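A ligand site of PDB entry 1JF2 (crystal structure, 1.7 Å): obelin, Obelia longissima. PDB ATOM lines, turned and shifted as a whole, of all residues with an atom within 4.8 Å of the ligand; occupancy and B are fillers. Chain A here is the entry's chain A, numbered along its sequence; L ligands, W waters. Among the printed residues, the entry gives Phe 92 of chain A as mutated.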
ATOM      1  N   HIS A  22     -23.828 -18.879   6.279  1.00  0.00           N
ATOM      2  CA  HIS A  22     -23.852 -17.845   5.252  1.00  0.00           C
ATOM      3  C   HIS A  22     -25.190 -17.770   4.547  1.00  0.00           C
ATOM      4  O   HIS A  22     -25.581 -16.713   4.060  1.00  0.00           O
ATOM      5  CB  HIS A  22     -22.706 -18.055   4.283  1.00  0.00           C
ATOM      6  CG  HIS A  22     -21.369 -17.796   4.907  1.00  0.00           C
ATOM      7  ND1 HIS A  22     -20.985 -16.529   5.304  1.00  0.00           N
ATOM      8  CD2 HIS A  22     -20.399 -18.640   5.330  1.00  0.00           C
ATOM      9  CE1 HIS A  22     -19.835 -16.612   5.946  1.00  0.00           C
ATOM     10  NE2 HIS A  22     -19.457 -17.871   5.982  1.00  0.00           N
ATOM     11  N   MET A  25     -27.087 -15.514   6.634  1.00  0.00           N
ATOM     12  CA  MET A  25     -26.719 -14.128   6.412  1.00  0.00           C
ATOM     13  C   MET A  25     -27.239 -13.620   5.079  1.00  0.00           C
ATOM     14  O   MET A  25     -27.697 -12.483   4.975  1.00  0.00           O
ATOM     15  CB  MET A  25     -25.189 -13.951   6.469  1.00  0.00           C
ATOM     16  CG  MET A  25     -24.597 -14.180   7.860  1.00  0.00           C
ATOM     17  SD  MET A  25     -25.385 -13.235   9.186  1.00  0.00           S
ATOM     18  CE  MET A  25     -25.016 -11.552   8.709  1.00  0.00           C
ATOM     19  N   PHE A  28     -30.819 -12.896   5.271  1.00  0.00           N
ATOM     20  CA  PHE A  28     -30.985 -11.738   6.131  1.00  0.00           C
ATOM     21  C   PHE A  28     -30.765 -10.447   5.338  1.00  0.00           C
ATOM     22  O   PHE A  28     -31.381  -9.412   5.611  1.00  0.00           O
ATOM     23  CB  PHE A  28     -29.980 -11.837   7.287  1.00  0.00           C
ATOM     24  CG  PHE A  28     -29.697 -10.538   7.972  1.00  0.00           C
ATOM     25  CD1 PHE A  28     -30.670  -9.900   8.733  1.00  0.00           C
ATOM     26  CD2 PHE A  28     -28.436  -9.954   7.866  1.00  0.00           C
ATOM     27  CE1 PHE A  28     -30.389  -8.703   9.378  1.00  0.00           C
ATOM     28  CE2 PHE A  28     -28.146  -8.750   8.504  1.00  0.00           C
ATOM     29  CZ  PHE A  28     -29.131  -8.122   9.263  1.00  0.00           C
ATOM     30  N   LEU A  29     -29.889 -10.513   4.330  1.00  0.00           N
ATOM     31  CA  LEU A  29     -29.603  -9.351   3.487  1.00  0.00           C
ATOM     32  C   LEU A  29     -30.571  -9.259   2.317  1.00  0.00           C
ATOM     33  O   LEU A  29     -30.729  -8.188   1.721  1.00  0.00           O
ATOM     34  CB  LEU A  29     -28.170  -9.429   2.953  1.00  0.00           C
ATOM     35  CG  LEU A  29     -27.046  -9.253   3.972  1.00  0.00           C
ATOM     36  CD1 LEU A  29     -25.702  -9.469   3.300  1.00  0.00           C
ATOM     37  CD2 LEU A  29     -27.130  -7.861   4.590  1.00  0.00           C
ATOM     38  N   ILE A  42     -26.657  -3.352   0.142  1.00  0.00           N
ATOM     39  CA  ILE A  42     -25.758  -3.592   1.259  1.00  0.00           C
ATOM     40  C   ILE A  42     -25.094  -2.306   1.755  1.00  0.00           C
ATOM     41  O   ILE A  42     -25.055  -2.050   2.964  1.00  0.00           O
ATOM     42  CB  ILE A  42     -24.664  -4.615   0.894  1.00  0.00           C
ATOM     43  CG1 ILE A  42     -25.272  -6.020   0.860  1.00  0.00           C
ATOM     44  CG2 ILE A  42     -23.526  -4.555   1.893  1.00  0.00           C
ATOM     45  CD1 ILE A  42     -24.286  -7.096   0.436  1.00  0.00           C
ATOM     46  N   LYS A  45     -27.549   0.000   3.517  1.00  0.00           N
ATOM     47  CA  LYS A  45     -27.802  -0.451   4.874  1.00  0.00           C
ATOM     48  C   LYS A  45     -26.726   0.086   5.821  1.00  0.00           C
ATOM     49  O   LYS A  45     -27.022   0.615   6.902  1.00  0.00           O
ATOM     50  CB  LYS A  45     -27.798  -1.985   4.917  1.00  0.00           C
ATOM     51  CG  LYS A  45     -27.987  -2.602   6.296  1.00  0.00           C
ATOM     52  CD  LYS A  45     -27.910  -4.126   6.210  1.00  0.00           C
ATOM     53  CE  LYS A  45     -28.110  -4.807   7.562  1.00  0.00           C
ATOM     54  NZ  LYS A  45     -29.489  -4.612   8.095  1.00  0.00           N
ATOM     55  N   ALA A  46     -25.480  -0.059   5.399  1.00  0.00           N
ATOM     56  CA  ALA A  46     -24.339   0.381   6.192  1.00  0.00           C
ATOM     57  C   ALA A  46     -24.306   1.889   6.433  1.00  0.00           C
ATOM     58  O   ALA A  46     -24.121   2.343   7.558  1.00  0.00           O
ATOM     59  CB  ALA A  46     -23.046  -0.058   5.524  1.00  0.00           C
ATOM     60  N   ILE A  50     -27.469   2.096   9.356  1.00  0.00           N
ATOM     61  CA  ILE A  50     -26.584   1.863  10.489  1.00  0.00           C
ATOM     62  C   ILE A  50     -25.797   3.093  10.963  1.00  0.00           C
ATOM     63  O   ILE A  50     -25.925   3.505  12.117  1.00  0.00           O
ATOM     64  CB  ILE A  50     -25.603   0.713  10.200  1.00  0.00           C
ATOM     65  CG1 ILE A  50     -26.397  -0.589  10.059  1.00  0.00           C
ATOM     66  CG2 ILE A  50     -24.582   0.598  11.319  1.00  0.00           C
ATOM     67  CD1 ILE A  50     -25.574  -1.771   9.598  1.00  0.00           C
ATOM     68  N   HIS A  64     -16.328   3.638   7.134  1.00  0.00           N
ATOM     69  CA  HIS A  64     -17.126   2.421   7.310  1.00  0.00           C
ATOM     70  C   HIS A  64     -17.648   1.942   5.963  1.00  0.00           C
ATOM     71  O   HIS A  64     -17.651   0.742   5.683  1.00  0.00           O
ATOM     72  CB  HIS A  64     -18.293   2.714   8.269  1.00  0.00           C
ATOM     73  CG  HIS A  64     -19.116   1.507   8.604  1.00  0.00           C
ATOM     74  ND1 HIS A  64     -20.294   1.212   7.958  1.00  0.00           N
ATOM     75  CD2 HIS A  64     -18.931   0.528   9.514  1.00  0.00           C
ATOM     76  CE1 HIS A  64     -20.792   0.090   8.451  1.00  0.00           C
ATOM     77  NE2 HIS A  64     -19.984  -0.346   9.394  1.00  0.00           N
ATOM     78  N   VAL A  68     -16.971  -1.735   4.100  1.00  0.00           N
ATOM     79  CA  VAL A  68     -18.056  -2.614   3.671  1.00  0.00           C
ATOM     80  C   VAL A  68     -17.930  -2.925   2.177  1.00  0.00           C
ATOM     81  O   VAL A  68     -18.058  -4.075   1.771  1.00  0.00           O
ATOM     82  CB  VAL A  68     -19.429  -1.974   3.973  1.00  0.00           C
ATOM     83  CG1 VAL A  68     -20.547  -2.819   3.383  1.00  0.00           C
ATOM     84  CG2 VAL A  68     -19.625  -1.865   5.495  1.00  0.00           C
ATOM     85  N   PHE A  71     -15.182  -5.469   1.677  1.00  0.00           N
ATOM     86  CA  PHE A  71     -15.579  -6.782   2.187  1.00  0.00           C
ATOM     87  C   PHE A  71     -16.473  -7.509   1.184  1.00  0.00           C
ATOM     88  O   PHE A  71     -16.199  -8.651   0.803  1.00  0.00           O
ATOM     89  CB  PHE A  71     -16.343  -6.628   3.505  1.00  0.00           C
ATOM     90  CG  PHE A  71     -16.659  -7.935   4.197  1.00  0.00           C
ATOM     91  CD1 PHE A  71     -15.741  -8.540   5.052  1.00  0.00           C
ATOM     92  CD2 PHE A  71     -17.903  -8.538   4.013  1.00  0.00           C
ATOM     93  CE1 PHE A  71     -16.055  -9.727   5.720  1.00  0.00           C
ATOM     94  CE2 PHE A  71     -18.226  -9.724   4.685  1.00  0.00           C
ATOM     95  CZ  PHE A  71     -17.296 -10.318   5.541  1.00  0.00           C
ATOM     96  N   PHE A  72     -17.537  -6.851   0.746  1.00  0.00           N
ATOM     97  CA  PHE A  72     -18.439  -7.502  -0.201  1.00  0.00           C
ATOM     98  C   PHE A  72     -17.944  -7.567  -1.642  1.00  0.00           C
ATOM     99  O   PHE A  72     -18.310  -8.480  -2.392  1.00  0.00           O
ATOM    100  CB  PHE A  72     -19.825  -6.876  -0.098  1.00  0.00           C
ATOM    101  CG  PHE A  72     -20.530  -7.221   1.189  1.00  0.00           C
ATOM    102  CD1 PHE A  72     -20.506  -6.333   2.254  1.00  0.00           C
ATOM    103  CD2 PHE A  72     -21.130  -8.460   1.355  1.00  0.00           C
ATOM    104  CE1 PHE A  72     -21.072  -6.675   3.477  1.00  0.00           C
ATOM    105  CE2 PHE A  72     -21.697  -8.822   2.586  1.00  0.00           C
ATOM    106  CZ  PHE A  72     -21.663  -7.926   3.643  1.00  0.00           C
ATOM    107  N   PHE A  88     -22.640 -16.023  -4.502  1.00  0.00           N
ATOM    108  CA  PHE A  88     -22.219 -15.239  -3.343  1.00  0.00           C
ATOM    109  C   PHE A  88     -21.346 -16.115  -2.444  1.00  0.00           C
ATOM    110  O   PHE A  88     -20.348 -15.650  -1.899  1.00  0.00           O
ATOM    111  CB  PHE A  88     -23.429 -14.774  -2.524  1.00  0.00           C
ATOM    112  CG  PHE A  88     -23.064 -14.133  -1.215  1.00  0.00           C
ATOM    113  CD1 PHE A  88     -22.564 -12.834  -1.185  1.00  0.00           C
ATOM    114  CD2 PHE A  88     -23.177 -14.837  -0.022  1.00  0.00           C
ATOM    115  CE1 PHE A  88     -22.170 -12.253   0.030  1.00  0.00           C
ATOM    116  CE2 PHE A  88     -22.787 -14.269   1.188  1.00  0.00           C
ATOM    117  CZ  PHE A  88     -22.290 -12.973   1.209  1.00  0.00           C
ATOM    118  N   PHE A  92     -17.594 -15.780  -1.239  1.00  0.00           N
ATOM    119  CA  PHE A  92     -17.194 -15.718   0.160  1.00  0.00           C
ATOM    120  C   PHE A  92     -16.014 -16.659   0.411  1.00  0.00           C
ATOM    121  O   PHE A  92     -15.155 -16.364   1.247  1.00  0.00           O
ATOM    122  CB  PHE A  92     -18.357 -16.077   1.077  1.00  0.00           C
ATOM    123  CG  PHE A  92     -18.277 -15.403   2.420  1.00  0.00           C
ATOM    124  CD1 PHE A  92     -18.902 -14.184   2.639  1.00  0.00           C
ATOM    125  CD2 PHE A  92     -17.502 -15.946   3.443  1.00  0.00           C
ATOM    126  CE1 PHE A  92     -18.759 -13.497   3.856  1.00  0.00           C
ATOM    127  CE2 PHE A  92     -17.341 -15.272   4.657  1.00  0.00           C
ATOM    128  CZ  PHE A  92     -17.979 -14.036   4.863  1.00  0.00           C
ATOM    129  N   ILE A 111     -11.867  -7.887   7.544  1.00  0.00           N
ATOM    130  CA  ILE A 111     -12.770  -7.932   8.677  1.00  0.00           C
ATOM    131  C   ILE A 111     -12.177  -7.153   9.864  1.00  0.00           C
ATOM    132  O   ILE A 111     -12.916  -6.563  10.632  1.00  0.00           O
ATOM    133  CB  ILE A 111     -13.142  -9.399   9.072  1.00  0.00           C
ATOM    134  CG1 ILE A 111     -14.270  -9.383  10.096  1.00  0.00           C
ATOM    135  CG2 ILE A 111     -11.935 -10.141   9.582  1.00  0.00           C
ATOM    136  CD1 ILE A 111     -15.558  -8.753   9.596  1.00  0.00           C
ATOM    137  N   TRP A 114     -12.798  -3.495   8.990  1.00  0.00           N
ATOM    138  CA  TRP A 114     -14.214  -3.166   9.129  1.00  0.00           C
ATOM    139  C   TRP A 114     -14.448  -2.979  10.627  1.00  0.00           C
ATOM    140  O   TRP A 114     -15.162  -2.074  11.052  1.00  0.00           O
ATOM    141  CB  TRP A 114     -15.073  -4.319   8.600  1.00  0.00           C
ATOM    142  CG  TRP A 114     -16.563  -4.063   8.578  1.00  0.00           C
ATOM    143  CD1 TRP A 114     -17.225  -2.969   9.048  1.00  0.00           C
ATOM    144  CD2 TRP A 114     -17.576  -4.958   8.088  1.00  0.00           C
ATOM    145  NE1 TRP A 114     -18.582  -3.126   8.893  1.00  0.00           N
ATOM    146  CE2 TRP A 114     -18.822  -4.334   8.304  1.00  0.00           C
ATOM    147  CE3 TRP A 114     -17.547  -6.230   7.496  1.00  0.00           C
ATOM    148  CZ2 TRP A 114     -20.036  -4.943   7.946  1.00  0.00           C
ATOM    149  CZ3 TRP A 114     -18.757  -6.827   7.143  1.00  0.00           C
ATOM    150  CH2 TRP A 114     -19.986  -6.180   7.365  1.00  0.00           C
ATOM    151  N   GLY A 115     -13.819  -3.846  11.421  1.00  0.00           N
ATOM    152  CA  GLY A 115     -13.942  -3.752  12.858  1.00  0.00           C
ATOM    153  C   GLY A 115     -13.449  -2.413  13.364  1.00  0.00           C
ATOM    154  O   GLY A 115     -14.106  -1.764  14.177  1.00  0.00           O
ATOM    155  N   VAL A 118     -16.047   0.177  12.861  1.00  0.00           N
ATOM    156  CA  VAL A 118     -17.205   0.093  13.740  1.00  0.00           C
ATOM    157  C   VAL A 118     -16.808   0.562  15.135  1.00  0.00           C
ATOM    158  O   VAL A 118     -17.519   1.337  15.773  1.00  0.00           O
ATOM    159  CB  VAL A 118     -17.764  -1.342  13.823  1.00  0.00           C
ATOM    160  CG1 VAL A 118     -18.831  -1.429  14.918  1.00  0.00           C
ATOM    161  CG2 VAL A 118     -18.373  -1.726  12.490  1.00  0.00           C
ATOM    162  N   PHE A 119     -15.650   0.081  15.590  1.00  0.00           N
ATOM    163  CA  PHE A 119     -15.149   0.442  16.911  1.00  0.00           C
ATOM    164  C   PHE A 119     -14.928   1.944  17.047  1.00  0.00           C
ATOM    165  O   PHE A 119     -15.178   2.518  18.112  1.00  0.00           O
ATOM    166  CB  PHE A 119     -13.828  -0.293  17.204  1.00  0.00           C
ATOM    167  CG  PHE A 119     -14.015  -1.633  17.851  1.00  0.00           C
ATOM    168  CD1 PHE A 119     -14.574  -2.693  17.150  1.00  0.00           C
ATOM    169  CD2 PHE A 119     -13.646  -1.826  19.177  1.00  0.00           C
ATOM    170  CE1 PHE A 119     -14.776  -3.937  17.767  1.00  0.00           C
ATOM    171  CE2 PHE A 119     -13.854  -3.056  19.802  1.00  0.00           C
ATOM    172  CZ  PHE A 119     -14.412  -4.106  19.098  1.00  0.00           C
ATOM    173  N   TRP A 135     -22.619  -2.644  22.016  1.00  0.00           N
ATOM    174  CA  TRP A 135     -22.802  -3.803  21.151  1.00  0.00           C
ATOM    175  C   TRP A 135     -24.293  -4.131  21.041  1.00  0.00           C
ATOM    176  O   TRP A 135     -24.770  -4.557  19.990  1.00  0.00           O
ATOM    177  CB  TRP A 135     -22.047  -5.010  21.671  1.00  0.00           C
ATOM    178  CG  TRP A 135     -22.183  -6.195  20.771  1.00  0.00           C
ATOM    179  CD1 TRP A 135     -22.879  -7.346  21.016  1.00  0.00           C
ATOM    180  CD2 TRP A 135     -21.656  -6.314  19.441  1.00  0.00           C
ATOM    181  NE1 TRP A 135     -22.816  -8.173  19.923  1.00  0.00           N
ATOM    182  CE2 TRP A 135     -22.065  -7.575  18.948  1.00  0.00           C
ATOM    183  CE3 TRP A 135     -20.877  -5.489  18.633  1.00  0.00           C
ATOM    184  CZ2 TRP A 135     -21.722  -8.015  17.662  1.00  0.00           C
ATOM    185  CZ3 TRP A 135     -20.530  -5.935  17.359  1.00  0.00           C
ATOM    186  CH2 TRP A 135     -20.958  -7.184  16.894  1.00  0.00           C
ATOM    187  N   TYR A 138     -25.564  -2.001  18.422  1.00  0.00           N
ATOM    188  CA  TYR A 138     -25.161  -2.466  17.106  1.00  0.00           C
ATOM    189  C   TYR A 138     -25.998  -3.664  16.654  1.00  0.00           C
ATOM    190  O   TYR A 138     -26.444  -3.721  15.505  1.00  0.00           O
ATOM    191  CB  TYR A 138     -23.689  -2.875  17.066  1.00  0.00           C
ATOM    192  CG  TYR A 138     -23.279  -3.254  15.668  1.00  0.00           C
ATOM    193  CD1 TYR A 138     -23.087  -2.281  14.696  1.00  0.00           C
ATOM    194  CD2 TYR A 138     -23.194  -4.595  15.287  1.00  0.00           C
ATOM    195  CE1 TYR A 138     -22.848  -2.615  13.369  1.00  0.00           C
ATOM    196  CE2 TYR A 138     -22.959  -4.951  13.959  1.00  0.00           C
ATOM    197  CZ  TYR A 138     -22.787  -3.957  13.010  1.00  0.00           C
ATOM    198  OH  TYR A 138     -22.616  -4.300  11.682  1.00  0.00           O
ATOM    199  N   ILE A 144     -28.422  -7.782  12.892  1.00  0.00           N
ATOM    200  CA  ILE A 144     -27.780  -9.091  12.933  1.00  0.00           C
ATOM    201  C   ILE A 144     -28.076  -9.842  14.238  1.00  0.00           C
ATOM    202  O   ILE A 144     -28.174 -11.069  14.232  1.00  0.00           O
ATOM    203  CB  ILE A 144     -26.256  -8.961  12.767  1.00  0.00           C
ATOM    204  CG1 ILE A 144     -25.637 -10.339  12.496  1.00  0.00           C
ATOM    205  CG2 ILE A 144     -25.641  -8.363  14.015  1.00  0.00           C
ATOM    206  CD1 ILE A 144     -24.166 -10.274  12.135  1.00  0.00           C
ATOM    207  N   VAL A 168     -11.109  -4.901  19.755  1.00  0.00           N
ATOM    208  CA  VAL A 168     -11.106  -5.265  18.336  1.00  0.00           C
ATOM    209  C   VAL A 168     -10.285  -6.500  17.955  1.00  0.00           C
ATOM    210  O   VAL A 168     -10.597  -7.184  16.976  1.00  0.00           O
ATOM    211  CB  VAL A 168     -10.673  -4.058  17.456  1.00  0.00           C
ATOM    212  CG1 VAL A 168      -9.187  -3.805  17.620  1.00  0.00           C
ATOM    213  CG2 VAL A 168     -11.035  -4.326  16.002  1.00  0.00           C
ATOM    214  N   MET A 171     -12.558  -9.490  18.885  1.00  0.00           N
ATOM    215  CA  MET A 171     -13.665  -9.624  17.947  1.00  0.00           C
ATOM    216  C   MET A 171     -13.171 -10.072  16.573  1.00  0.00           C
ATOM    217  O   MET A 171     -13.821 -10.876  15.908  1.00  0.00           O
ATOM    218  CB  MET A 171     -14.461  -8.324  17.816  1.00  0.00           C
ATOM    219  CG  MET A 171     -15.834  -8.549  17.195  1.00  0.00           C
ATOM    220  SD  MET A 171     -16.749  -9.856  18.052  1.00  0.00           S
ATOM    221  CE  MET A 171     -18.455  -9.343  17.738  1.00  0.00           C
ATOM    222  N   THR A 172     -12.017  -9.563  16.136  1.00  0.00           N
ATOM    223  CA  THR A 172     -11.462  -9.950  14.838  1.00  0.00           C
ATOM    224  C   THR A 172     -11.144 -11.450  14.832  1.00  0.00           C
ATOM    225  O   THR A 172     -11.464 -12.174  13.883  1.00  0.00           O
ATOM    226  CB  THR A 172     -10.163  -9.166  14.534  1.00  0.00           C
ATOM    227  OG1 THR A 172     -10.469  -7.770  14.390  1.00  0.00           O
ATOM    228  CG2 THR A 172      -9.508  -9.672  13.272  1.00  0.00           C
ATOM    229  N   HIS A 175     -14.336 -13.385  14.712  1.00  0.00           N
ATOM    230  CA  HIS A 175     -14.935 -13.278  13.394  1.00  0.00           C
ATOM    231  C   HIS A 175     -14.205 -14.065  12.323  1.00  0.00           C
ATOM    232  O   HIS A 175     -14.841 -14.599  11.420  1.00  0.00           O
ATOM    233  CB  HIS A 175     -15.037 -11.804  12.977  1.00  0.00           C
ATOM    234  CG  HIS A 175     -16.292 -11.128  13.432  1.00  0.00           C
ATOM    235  ND1 HIS A 175     -16.428  -9.762  13.467  1.00  0.00           N
ATOM    236  CD2 HIS A 175     -17.476 -11.634  13.846  1.00  0.00           C
ATOM    237  CE1 HIS A 175     -17.649  -9.451  13.873  1.00  0.00           C
ATOM    238  NE2 HIS A 175     -18.308 -10.572  14.113  1.00  0.00           N
ATOM    239  N   TRP A 179     -16.753 -16.459  10.544  1.00  0.00           N
ATOM    240  CA  TRP A 179     -17.103 -16.298   9.140  1.00  0.00           C
ATOM    241  C   TRP A 179     -16.278 -17.142   8.177  1.00  0.00           C
ATOM    242  O   TRP A 179     -16.794 -17.645   7.173  1.00  0.00           O
ATOM    243  CB  TRP A 179     -16.949 -14.825   8.713  1.00  0.00           C
ATOM    244  CG  TRP A 179     -17.803 -13.836   9.472  1.00  0.00           C
ATOM    245  CD1 TRP A 179     -17.400 -12.634   9.978  1.00  0.00           C
ATOM    246  CD2 TRP A 179     -19.190 -13.962   9.795  1.00  0.00           C
ATOM    247  NE1 TRP A 179     -18.451 -11.999  10.590  1.00  0.00           N
ATOM    248  CE2 TRP A 179     -19.568 -12.788  10.489  1.00  0.00           C
ATOM    249  CE3 TRP A 179     -20.168 -14.951   9.559  1.00  0.00           C
ATOM    250  CZ2 TRP A 179     -20.870 -12.579  10.959  1.00  0.00           C
ATOM    251  CZ3 TRP A 179     -21.461 -14.734  10.021  1.00  0.00           C
ATOM    252  CH2 TRP A 179     -21.798 -13.554  10.706  1.00  0.00           C
ATOM    253  N   TYR A 190     -22.639 -15.401  18.327  1.00  0.00           N
ATOM    254  CA  TYR A 190     -23.833 -14.559  18.261  1.00  0.00           C
ATOM    255  C   TYR A 190     -25.052 -15.133  18.960  1.00  0.00           C
ATOM    256  O   TYR A 190     -26.178 -14.769  18.618  1.00  0.00           O
ATOM    257  CB  TYR A 190     -24.205 -14.280  16.798  1.00  0.00           C
ATOM    258  CG  TYR A 190     -23.350 -13.236  16.139  1.00  0.00           C
ATOM    259  CD1 TYR A 190     -22.117 -13.577  15.577  1.00  0.00           C
ATOM    260  CD2 TYR A 190     -23.738 -11.903  16.126  1.00  0.00           C
ATOM    261  CE1 TYR A 190     -21.297 -12.596  15.028  1.00  0.00           C
ATOM    262  CE2 TYR A 190     -22.931 -10.923  15.572  1.00  0.00           C
ATOM    263  CZ  TYR A 190     -21.714 -11.276  15.033  1.00  0.00           C
ATOM    264  OH  TYR A 190     -20.901 -10.300  14.524  1.00  0.00           O
HETATM  265  N1  LIG L   1     -21.754  -6.713  10.922  1.00  0.00           N
HETATM  266  C1  LIG L   1     -20.577  -6.954  11.683  1.00  0.00           C
HETATM  267  C2  LIG L   1     -20.006  -8.262  10.965  1.00  0.00           C
HETATM  268  N2  LIG L   1     -20.829  -8.586  10.008  1.00  0.00           N
HETATM  269  C3  LIG L   1     -20.720  -9.746   9.057  1.00  0.00           C
HETATM  270  C4  LIG L   1     -21.728  -9.872   8.118  1.00  0.00           C
HETATM  271  N3  LIG L   1     -22.850  -8.861   8.129  1.00  0.00           N
HETATM  272  C5  LIG L   1     -22.918  -7.824   8.991  1.00  0.00           C
HETATM  273  C6  LIG L   1     -21.830  -7.658  10.007  1.00  0.00           C
HETATM  274  C7  LIG L   1     -19.589  -5.726  11.602  1.00  0.00           C
HETATM  275  C8  LIG L   1     -18.343  -5.909  12.461  1.00  0.00           C
HETATM  276  C9  LIG L   1     -18.403  -5.682  13.911  1.00  0.00           C
HETATM  277  C10 LIG L   1     -17.235  -5.847  14.727  1.00  0.00           C
HETATM  278  C11 LIG L   1     -15.990  -6.252  14.114  1.00  0.00           C
HETATM  279  C12 LIG L   1     -15.917  -6.487  12.673  1.00  0.00           C
HETATM  280  C13 LIG L   1     -17.098  -6.305  11.844  1.00  0.00           C
HETATM  281  O1  LIG L   1     -14.918  -6.405  14.900  1.00  0.00           O
HETATM  282  O2  LIG L   1     -18.983  -8.855  11.291  1.00  0.00           O
HETATM  283  C14 LIG L   1     -21.823 -10.961   7.139  1.00  0.00           C
HETATM  284  C15 LIG L   1     -22.660 -10.799   5.966  1.00  0.00           C
HETATM  285  C16 LIG L   1     -22.775 -11.886   5.018  1.00  0.00           C
HETATM  286  C17 LIG L   1     -22.055 -13.128   5.231  1.00  0.00           C
HETATM  287  C18 LIG L   1     -21.222 -13.284   6.392  1.00  0.00           C
HETATM  288  C19 LIG L   1     -21.106 -12.225   7.327  1.00  0.00           C
HETATM  289  O3  LIG L   1     -22.184 -14.134   4.351  1.00  0.00           O
HETATM  290  C20 LIG L   1     -24.099  -6.890   8.884  1.00  0.00           C
HETATM  291  C21 LIG L   1     -23.998  -5.883   7.800  1.00  0.00           C
HETATM  292  C22 LIG L   1     -23.734  -4.497   8.135  1.00  0.00           C
HETATM  293  C23 LIG L   1     -23.635  -3.491   7.076  1.00  0.00           C
HETATM  294  C24 LIG L   1     -23.796  -3.877   5.693  1.00  0.00           C
HETATM  295  C25 LIG L   1     -24.059  -5.263   5.358  1.00  0.00           C
HETATM  296  C26 LIG L   1     -24.157  -6.268   6.393  1.00  0.00           C
HETATM  297  O4  LIG L   1     -21.089  -7.086  13.033  1.00  0.00           O
HETATM  298  O5  LIG L   1     -21.870  -8.258  12.976  1.00  0.00           O
HETATM  299  O   HOH W   1     -21.861  -2.375   9.985  1.00  0.00           O
HETATM  300  O   HOH W   2     -12.815  -7.374  13.246  1.00  0.00           O
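N1 of the ligand sits at hydrogen-bond distance from OH of Tyr 138, at 2.7 Å. O5 of the ligand lies within hydrogen-bond range of OH of Tyr 190 (2.7 Å). ND1 of His 22 lies within hydrogen-bond range of O3 of the ligand (2.8 Å). NE2 of His 175 sits close to O2 of the ligand, 3.4 Å away. The indole nitrogen of Trp 179 lies within hydrogen-bond range of an oxygen (O2) of the ligand.
The side-chain hydroxyl (OH) of Tyr 190 is in hydrogen-bond range of a ring nitrogen (NE2) of His 175 (2.6 Å). The backbone carbonyl oxygen (O) of Trp 179 lies within hydrogen-bond range of a ring nitrogen (NE2) of His 22 (2.9 Å). A ring nitrogen (NE2) of His 64 is in hydrogen-bond range of the indole nitrogen of Trp 114 (3.2 Å). The backbone NH of Ile 50 is in hydrogen-bond range of the backbone carbonyl oxygen of Lys 45 (2.9 Å).
Water W2 lies within hydrogen-bond range of OG1 of Thr 172 (2.6 Å), O of Ile 111 (2.7 Å) and O1 of the ligand (2.8 Å). Water W1 bridges the side-chain hydroxyl of Tyr 138 (2.7 Å) and a ring nitrogen (NE2) of His 64 (2.8 Å).
Merely in contact with the ligand: Ile 144 (3.2 Å), Phe 88 (3.2 Å), Met 171 (3.3 Å), Gly 115 (3.4 Å), Met 25 (3.5 Å), Ile 42 (3.5 Å), Phe 92 (3.5 Å), Trp 114 (3.5 Å), Ile 50 (3.6 Å), Ile 111 (3.6 Å), Phe 119 (3.8 Å), Phe 72 (3.8 Å), Ala 46 (3.8 Å), Leu 29 (3.8 Å) and Trp 135 (3.9 Å). Hydrophobic or aromatic side chains that line the ligand: His 22, Met 25, Leu 29, Ile 42, Ala 46, Ile 50, Phe 72, Phe 88, Phe 92, Ile 111, Trp 114, Phe 119, Trp 135, Tyr 138, Ile 144, Met 171, His 175, Trp 179 and Tyr 190. 20 residues have an atom within 4 Å of the ligand: His 22, Met 25, Leu 29, Ile 42, Ala 46, Ile 50, Phe 72, Phe 88, Phe 92, Ile 111, Trp 114, Gly 115, Phe 119, Trp 135, Tyr 138, Ile 144, Met 171, His 175, Trp 179 and Tyr 190.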
